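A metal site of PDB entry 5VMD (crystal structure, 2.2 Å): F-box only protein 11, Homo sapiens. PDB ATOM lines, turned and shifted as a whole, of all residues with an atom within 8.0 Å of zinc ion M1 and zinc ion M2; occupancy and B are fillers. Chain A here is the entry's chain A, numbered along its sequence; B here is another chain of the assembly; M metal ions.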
ATOM      1  N   ALA A  36      -1.336 -25.749 -25.703  1.00  0.00           N
ATOM      2  CA  ALA A  36      -2.165 -24.572 -25.518  1.00  0.00           C
ATOM      3  C   ALA A  36      -2.516 -24.445 -24.043  1.00  0.00           C
ATOM      4  O   ALA A  36      -3.059 -25.377 -23.441  1.00  0.00           O
ATOM      5  CB  ALA A  36      -3.440 -24.651 -26.375  1.00  0.00           C
ATOM      6  N   ILE A  37      -2.245 -23.278 -23.477  1.00  0.00           N
ATOM      7  CA  ILE A  37      -2.310 -23.029 -22.041  1.00  0.00           C
ATOM      8  C   ILE A  37      -3.092 -21.752 -21.794  1.00  0.00           C
ATOM      9  O   ILE A  37      -2.894 -20.756 -22.500  1.00  0.00           O
ATOM     10  CB  ILE A  37      -0.892 -22.939 -21.460  1.00  0.00           C
ATOM     11  CG1 ILE A  37      -0.127 -24.246 -21.735  1.00  0.00           C
ATOM     12  CG2 ILE A  37      -0.934 -22.575 -19.963  1.00  0.00           C
ATOM     13  CD1 ILE A  37       1.363 -24.161 -21.496  1.00  0.00           C
ATOM     14  N   CYS A  38      -3.969 -21.768 -20.789  1.00  0.00           N
ATOM     15  CA  CYS A  38      -4.776 -20.604 -20.450  1.00  0.00           C
ATOM     16  C   CYS A  38      -3.943 -19.557 -19.715  1.00  0.00           C
ATOM     17  O   CYS A  38      -2.845 -19.829 -19.236  1.00  0.00           O
ATOM     18  CB  CYS A  38      -5.985 -21.016 -19.597  1.00  0.00           C
ATOM     19  SG  CYS A  38      -5.591 -21.501 -17.881  1.00  0.00           S
ATOM     20  N   VAL A  39      -4.490 -18.338 -19.646  1.00  0.00           N
ATOM     21  CA  VAL A  39      -3.750 -17.214 -19.067  1.00  0.00           C
ATOM     22  C   VAL A  39      -3.493 -17.448 -17.587  1.00  0.00           C
ATOM     23  O   VAL A  39      -2.417 -17.120 -17.070  1.00  0.00           O
ATOM     24  CB  VAL A  39      -4.503 -15.885 -19.301  1.00  0.00           C
ATOM     25  CG1 VAL A  39      -5.865 -15.916 -18.636  1.00  0.00           C
ATOM     26  CG2 VAL A  39      -3.684 -14.723 -18.751  1.00  0.00           C
ATOM     27  N   ASN A  40      -4.478 -17.999 -16.871  1.00  0.00           N
ATOM     28  CA  ASN A  40      -4.295 -18.274 -15.451  1.00  0.00           C
ATOM     29  C   ASN A  40      -3.169 -19.279 -15.224  1.00  0.00           C
ATOM     30  O   ASN A  40      -2.359 -19.120 -14.306  1.00  0.00           O
ATOM     31  CB  ASN A  40      -5.618 -18.757 -14.854  1.00  0.00           C
ATOM     32  CG  ASN A  40      -6.612 -17.624 -14.652  1.00  0.00           C
ATOM     33  OD1 ASN A  40      -6.233 -16.453 -14.667  1.00  0.00           O
ATOM     34  ND2 ASN A  40      -7.883 -17.958 -14.498  1.00  0.00           N
ATOM     35  N   CYS A  41      -3.108 -20.332 -16.041  1.00  0.00           N
ATOM     36  CA  CYS A  41      -2.045 -21.315 -15.886  1.00  0.00           C
ATOM     37  C   CYS A  41      -0.692 -20.761 -16.281  1.00  0.00           C
ATOM     38  O   CYS A  41       0.318 -21.054 -15.633  1.00  0.00           O
ATOM     39  CB  CYS A  41      -2.360 -22.592 -16.674  1.00  0.00           C
ATOM     40  SG  CYS A  41      -3.581 -23.646 -15.877  1.00  0.00           S
ATOM     41  N   ILE A  42      -0.639 -19.935 -17.330  1.00  0.00           N
ATOM     42  CA  ILE A  42       0.671 -19.433 -17.749  1.00  0.00           C
ATOM     43  C   ILE A  42       1.278 -18.600 -16.640  1.00  0.00           C
ATOM     44  O   ILE A  42       2.502 -18.614 -16.446  1.00  0.00           O
ATOM     45  CB  ILE A  42       0.577 -18.655 -19.074  1.00  0.00           C
ATOM     46  CG1 ILE A  42       1.885 -18.815 -19.857  1.00  0.00           C
ATOM     47  CG2 ILE A  42       0.297 -17.164 -18.818  1.00  0.00           C
ATOM     48  CD1 ILE A  42       2.136 -20.273 -20.322  1.00  0.00           C
ATOM     49  N   LYS A  43       0.444 -17.883 -15.884  1.00  0.00           N
ATOM     50  CA  LYS A  43       0.924 -17.028 -14.798  1.00  0.00           C
ATOM     51  C   LYS A  43       1.314 -17.836 -13.567  1.00  0.00           C
ATOM     52  O   LYS A  43       2.372 -17.625 -12.981  1.00  0.00           O
ATOM     53  CB  LYS A  43      -0.147 -15.993 -14.426  1.00  0.00           C
ATOM     54  CG  LYS A  43      -0.475 -14.947 -15.487  1.00  0.00           C
ATOM     55  CD  LYS A  43      -1.348 -13.848 -14.878  1.00  0.00           C
ATOM     56  CE  LYS A  43      -1.369 -12.562 -15.698  1.00  0.00           C
ATOM     57  NZ  LYS A  43      -2.239 -12.622 -16.894  1.00  0.00           N
ATOM     58  N   LYS A  44       0.459 -18.772 -13.166  1.00  0.00           N
ATOM     59  CA  LYS A  44       0.692 -19.497 -11.917  1.00  0.00           C
ATOM     60  C   LYS A  44       1.429 -20.807 -12.114  1.00  0.00           C
ATOM     61  O   LYS A  44       2.169 -21.237 -11.207  1.00  0.00           O
ATOM     62  CB  LYS A  44      -0.635 -19.738 -11.209  1.00  0.00           C
ATOM     63  CG  LYS A  44      -1.325 -18.468 -10.772  1.00  0.00           C
ATOM     64  CD  LYS A  44      -0.392 -17.647  -9.900  1.00  0.00           C
ATOM     65  CE  LYS A  44      -1.023 -16.344  -9.437  1.00  0.00           C
ATOM     66  NZ  LYS A  44      -0.143 -15.606  -8.473  1.00  0.00           N
ATOM     67  N   CYS A  45       1.288 -21.450 -13.273  1.00  0.00           N
ATOM     68  CA  CYS A  45       1.884 -22.762 -13.497  1.00  0.00           C
ATOM     69  C   CYS A  45       3.147 -22.728 -14.336  1.00  0.00           C
ATOM     70  O   CYS A  45       3.864 -23.732 -14.370  1.00  0.00           O
ATOM     71  CB  CYS A  45       0.857 -23.700 -14.146  1.00  0.00           C
ATOM     72  SG  CYS A  45      -0.700 -23.810 -13.242  1.00  0.00           S
ATOM     73  N   HIS A  46       3.459 -21.612 -14.993  1.00  0.00           N
ATOM     74  CA  HIS A  46       4.629 -21.574 -15.878  1.00  0.00           C
ATOM     75  C   HIS A  46       5.428 -20.304 -15.650  1.00  0.00           C
ATOM     76  O   HIS A  46       6.080 -19.797 -16.573  1.00  0.00           O
ATOM     77  CB  HIS A  46       4.202 -21.745 -17.342  1.00  0.00           C
ATOM     78  CG  HIS A  46       3.418 -23.003 -17.580  1.00  0.00           C
ATOM     79  ND1 HIS A  46       4.005 -24.185 -17.989  1.00  0.00           N
ATOM     80  CD2 HIS A  46       2.101 -23.277 -17.412  1.00  0.00           C
ATOM     81  CE1 HIS A  46       3.085 -25.126 -18.089  1.00  0.00           C
ATOM     82  NE2 HIS A  46       1.920 -24.599 -17.732  1.00  0.00           N
ATOM     83  N   PHE B  59     -11.234 -23.175 -24.973  1.00  0.00           N
ATOM     84  CA  PHE B  59     -11.019 -23.288 -23.542  1.00  0.00           C
ATOM     85  C   PHE B  59     -10.132 -24.468 -23.167  1.00  0.00           C
ATOM     86  O   PHE B  59      -9.893 -24.680 -21.964  1.00  0.00           O
ATOM     87  CB  PHE B  59     -12.374 -23.383 -22.824  1.00  0.00           C
ATOM     88  CG  PHE B  59     -13.235 -22.186 -23.044  1.00  0.00           C
ATOM     89  CD1 PHE B  59     -12.824 -20.930 -22.611  1.00  0.00           C
ATOM     90  CD2 PHE B  59     -14.459 -22.300 -23.690  1.00  0.00           C
ATOM     91  CE1 PHE B  59     -13.621 -19.806 -22.820  1.00  0.00           C
ATOM     92  CE2 PHE B  59     -15.265 -21.179 -23.897  1.00  0.00           C
ATOM     93  CZ  PHE B  59     -14.841 -19.928 -23.460  1.00  0.00           C
ATOM     94  N   PHE B  60      -9.632 -25.236 -24.137  1.00  0.00           N
ATOM     95  CA  PHE B  60      -8.766 -26.353 -23.776  1.00  0.00           C
ATOM     96  C   PHE B  60      -7.437 -25.836 -23.263  1.00  0.00           C
ATOM     97  O   PHE B  60      -6.851 -24.907 -23.810  1.00  0.00           O
ATOM     98  CB  PHE B  60      -8.518 -27.276 -24.964  1.00  0.00           C
ATOM     99  CG  PHE B  60      -7.606 -28.429 -24.636  1.00  0.00           C
ATOM    100  CD1 PHE B  60      -8.110 -29.566 -24.020  1.00  0.00           C
ATOM    101  CD2 PHE B  60      -6.240 -28.352 -24.886  1.00  0.00           C
ATOM    102  CE1 PHE B  60      -7.262 -30.639 -23.694  1.00  0.00           C
ATOM    103  CE2 PHE B  60      -5.386 -29.416 -24.569  1.00  0.00           C
ATOM    104  CZ  PHE B  60      -5.902 -30.561 -23.972  1.00  0.00           C
ATOM    105  N   CYS B  61      -6.940 -26.471 -22.209  1.00  0.00           N
ATOM    106  CA  CYS B  61      -5.660 -26.101 -21.616  1.00  0.00           C
ATOM    107  C   CYS B  61      -4.865 -27.359 -21.336  1.00  0.00           C
ATOM    108  O   CYS B  61      -5.281 -28.181 -20.521  1.00  0.00           O
ATOM    109  CB  CYS B  61      -5.844 -25.299 -20.327  1.00  0.00           C
ATOM    110  SG  CYS B  61      -4.277 -24.959 -19.493  1.00  0.00           S
ATOM    111  N   ASP B  62      -3.722 -27.493 -22.002  1.00  0.00           N
ATOM    112  CA  ASP B  62      -2.859 -28.641 -21.757  1.00  0.00           C
ATOM    113  C   ASP B  62      -2.418 -28.715 -20.299  1.00  0.00           C
ATOM    114  O   ASP B  62      -2.250 -29.825 -19.773  1.00  0.00           O
ATOM    115  CB  ASP B  62      -1.648 -28.600 -22.694  1.00  0.00           C
ATOM    116  CG  ASP B  62      -1.971 -29.154 -24.062  1.00  0.00           C
ATOM    117  OD1 ASP B  62      -2.186 -30.374 -24.143  1.00  0.00           O
ATOM    118  OD2 ASP B  62      -1.997 -28.385 -25.054  1.00  0.00           O
ATOM    119  N   CYS B  63      -2.246 -27.571 -19.626  1.00  0.00           N
ATOM    120  CA  CYS B  63      -1.808 -27.602 -18.229  1.00  0.00           C
ATOM    121  C   CYS B  63      -2.896 -28.200 -17.350  1.00  0.00           C
ATOM    122  O   CYS B  63      -2.673 -29.211 -16.670  1.00  0.00           O
ATOM    123  CB  CYS B  63      -1.433 -26.191 -17.756  1.00  0.00           C
ATOM    124  SG  CYS B  63      -0.573 -26.135 -16.131  1.00  0.00           S
ATOM    125  N   GLY B  64      -4.091 -27.610 -17.381  1.00  0.00           N
ATOM    126  CA  GLY B  64      -5.191 -28.162 -16.604  1.00  0.00           C
ATOM    127  C   GLY B  64      -5.583 -29.554 -17.029  1.00  0.00           C
ATOM    128  O   GLY B  64      -6.094 -30.335 -16.212  1.00  0.00           O
ATOM    129  N   ALA B  65      -5.352 -29.905 -18.298  1.00  0.00           N
ATOM    130  CA  ALA B  65      -5.662 -31.254 -18.781  1.00  0.00           C
ATOM    131  C   ALA B  65      -4.675 -32.298 -18.295  1.00  0.00           C
ATOM    132  O   ALA B  65      -4.924 -33.500 -18.469  1.00  0.00           O
ATOM    133  CB  ALA B  65      -5.720 -31.279 -20.313  1.00  0.00           C
ATOM    134  N   GLY B  66      -3.555 -31.887 -17.701  1.00  0.00           N
ATOM    135  CA  GLY B  66      -2.577 -32.847 -17.193  1.00  0.00           C
ATOM    136  C   GLY B  66      -1.649 -33.448 -18.222  1.00  0.00           C
ATOM    137  O   GLY B  66      -1.122 -34.533 -17.988  1.00  0.00           O
ATOM    138  N   LEU B  68       1.149 -31.835 -19.396  1.00  0.00           N
ATOM    139  CA  LEU B  68       2.480 -31.262 -19.279  1.00  0.00           C
ATOM    140  C   LEU B  68       3.257 -32.006 -18.191  1.00  0.00           C
ATOM    141  O   LEU B  68       2.688 -32.729 -17.373  1.00  0.00           O
ATOM    142  CB  LEU B  68       2.388 -29.766 -18.968  1.00  0.00           C
ATOM    143  CG  LEU B  68       1.528 -29.021 -19.995  1.00  0.00           C
ATOM    144  CD1 LEU B  68       1.436 -27.536 -19.649  1.00  0.00           C
ATOM    145  CD2 LEU B  68       2.065 -29.210 -21.412  1.00  0.00           C
ATOM    146  N   ASN B  70       4.663 -31.088 -15.457  1.00  0.00           N
ATOM    147  CA  ASN B  70       4.292 -30.838 -14.071  1.00  0.00           C
ATOM    148  C   ASN B  70       2.776 -30.743 -13.915  1.00  0.00           C
ATOM    149  O   ASN B  70       2.091 -30.234 -14.807  1.00  0.00           O
ATOM    150  CB  ASN B  70       4.929 -29.541 -13.560  1.00  0.00           C
ATOM    151  CG  ASN B  70       6.446 -29.556 -13.653  1.00  0.00           C
ATOM    152  OD1 ASN B  70       7.084 -30.571 -13.395  1.00  0.00           O
ATOM    153  ND2 ASN B  70       7.028 -28.427 -14.040  1.00  0.00           N
ATOM    154  N   PRO B  71       2.217 -31.177 -12.789  1.00  0.00           N
ATOM    155  CA  PRO B  71       0.770 -31.076 -12.597  1.00  0.00           C
ATOM    156  C   PRO B  71       0.328 -29.625 -12.468  1.00  0.00           C
ATOM    157  O   PRO B  71       1.078 -28.765 -11.997  1.00  0.00           O
ATOM    158  CB  PRO B  71       0.518 -31.838 -11.284  1.00  0.00           C
ATOM    159  CG  PRO B  71       1.774 -32.663 -11.058  1.00  0.00           C
ATOM    160  CD  PRO B  71       2.879 -31.853 -11.658  1.00  0.00           C
ATOM    161  N   CYS B  72      -0.898 -29.355 -12.899  1.00  0.00           N
ATOM    162  CA  CYS B  72      -1.438 -27.996 -12.813  1.00  0.00           C
ATOM    163  C   CYS B  72      -1.595 -27.591 -11.354  1.00  0.00           C
ATOM    164  O   CYS B  72      -2.059 -28.377 -10.519  1.00  0.00           O
ATOM    165  CB  CYS B  72      -2.791 -27.922 -13.527  1.00  0.00           C
ATOM    166  SG  CYS B  72      -3.641 -26.325 -13.389  1.00  0.00           S
ATOM    167  N   THR B  73      -1.258 -26.345 -11.043  1.00  0.00           N
ATOM    168  CA  THR B  73      -1.367 -25.866  -9.668  1.00  0.00           C
ATOM    169  C   THR B  73      -2.728 -25.248  -9.379  1.00  0.00           C
ATOM    170  O   THR B  73      -2.990 -24.875  -8.233  1.00  0.00           O
ATOM    171  CB  THR B  73      -0.276 -24.832  -9.366  1.00  0.00           C
ATOM    172  OG1 THR B  73      -0.606 -23.577  -9.978  1.00  0.00           O
ATOM    173  CG2 THR B  73       1.062 -25.308  -9.902  1.00  0.00           C
ATOM    174  N   LEU B  74      -3.598 -25.171 -10.377  1.00  0.00           N
ATOM    175  CA  LEU B  74      -4.910 -24.554 -10.214  1.00  0.00           C
ATOM    176  C   LEU B  74      -6.032 -25.610 -10.163  1.00  0.00           C
ATOM    177  O   LEU B  74      -5.775 -26.813 -10.126  1.00  0.00           O
ATOM    178  CB  LEU B  74      -5.163 -23.568 -11.353  1.00  0.00           C
ATOM    179  CG  LEU B  74      -4.124 -22.444 -11.411  1.00  0.00           C
ATOM    180  CD1 LEU B  74      -4.382 -21.506 -12.589  1.00  0.00           C
ATOM    181  CD2 LEU B  74      -4.084 -21.664 -10.083  1.00  0.00           C
HETATM  182 ZN    ZN M   1      -2.122 -25.134 -14.740  1.00  0.00          ZN
HETATM  183 ZN    ZN M   2      -5.230 -23.861 -17.605  1.00  0.00          ZN
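SG of Cys 63 of chain B is bound to zinc ion M1 (2.3 Å). The side-chain sulfur (SG) of Cys 72 of chain B is bound to zinc ion M1 (2.4 Å). Zinc ion M1 is bound by SG of Cys 41 (2.4 Å). Zinc ion M1 is bound by SG of Cys 45, at 2.5 Å. Zinc ion M1 has four donor atoms within binding distance.
N of Thr 73 of chain B touches zinc ion M1, at 3.99 Å. Within 4 Å of zinc ion M1: Cys 41, Cys 45, Cys 63 of chain B, Cys 72 of chain B and Thr 73 of chain B. The nearest printed residue that does not touch zinc ion M1 is Gly 64 of chain B (4.1 Å).
The backbone NH of Cys 63 of chain B lies close to the side-chain sulfur of Cys 61 of chain B (3.3 Å). The side-chain sulfur (SG) of Cys 63 of chain B lies close to a ring nitrogen (NE2) of His 46 (3.3 Å). The backbone carbonyl oxygen (O) of Cys 41 is in hydrogen-bond range of the backbone NH (N) of His 46, 3.3 Å away. The backbone NH (N) of Gly 64 of chain B lies close to the side-chain sulfur (SG) of Cys 61 of chain B, 3.4 Å away. SG of Cys 45 lies close to OG1 of Thr 73 of chain B (3.3 Å). N of Leu 74 of chain B sits close to SG of Cys 72 of chain B (3.2 Å).
Zinc ion M2 is bound by SG of Cys 61 of chain B (2.4 Å), SG of Cys 41 (2.4 Å) and SG of Cys 38 (2.4 Å).
Gly 64 of chain B touches zinc ion M2. The nearest printed residue that does not touch zinc ion M2 is Cys 63 of chain B (4.5 Å).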
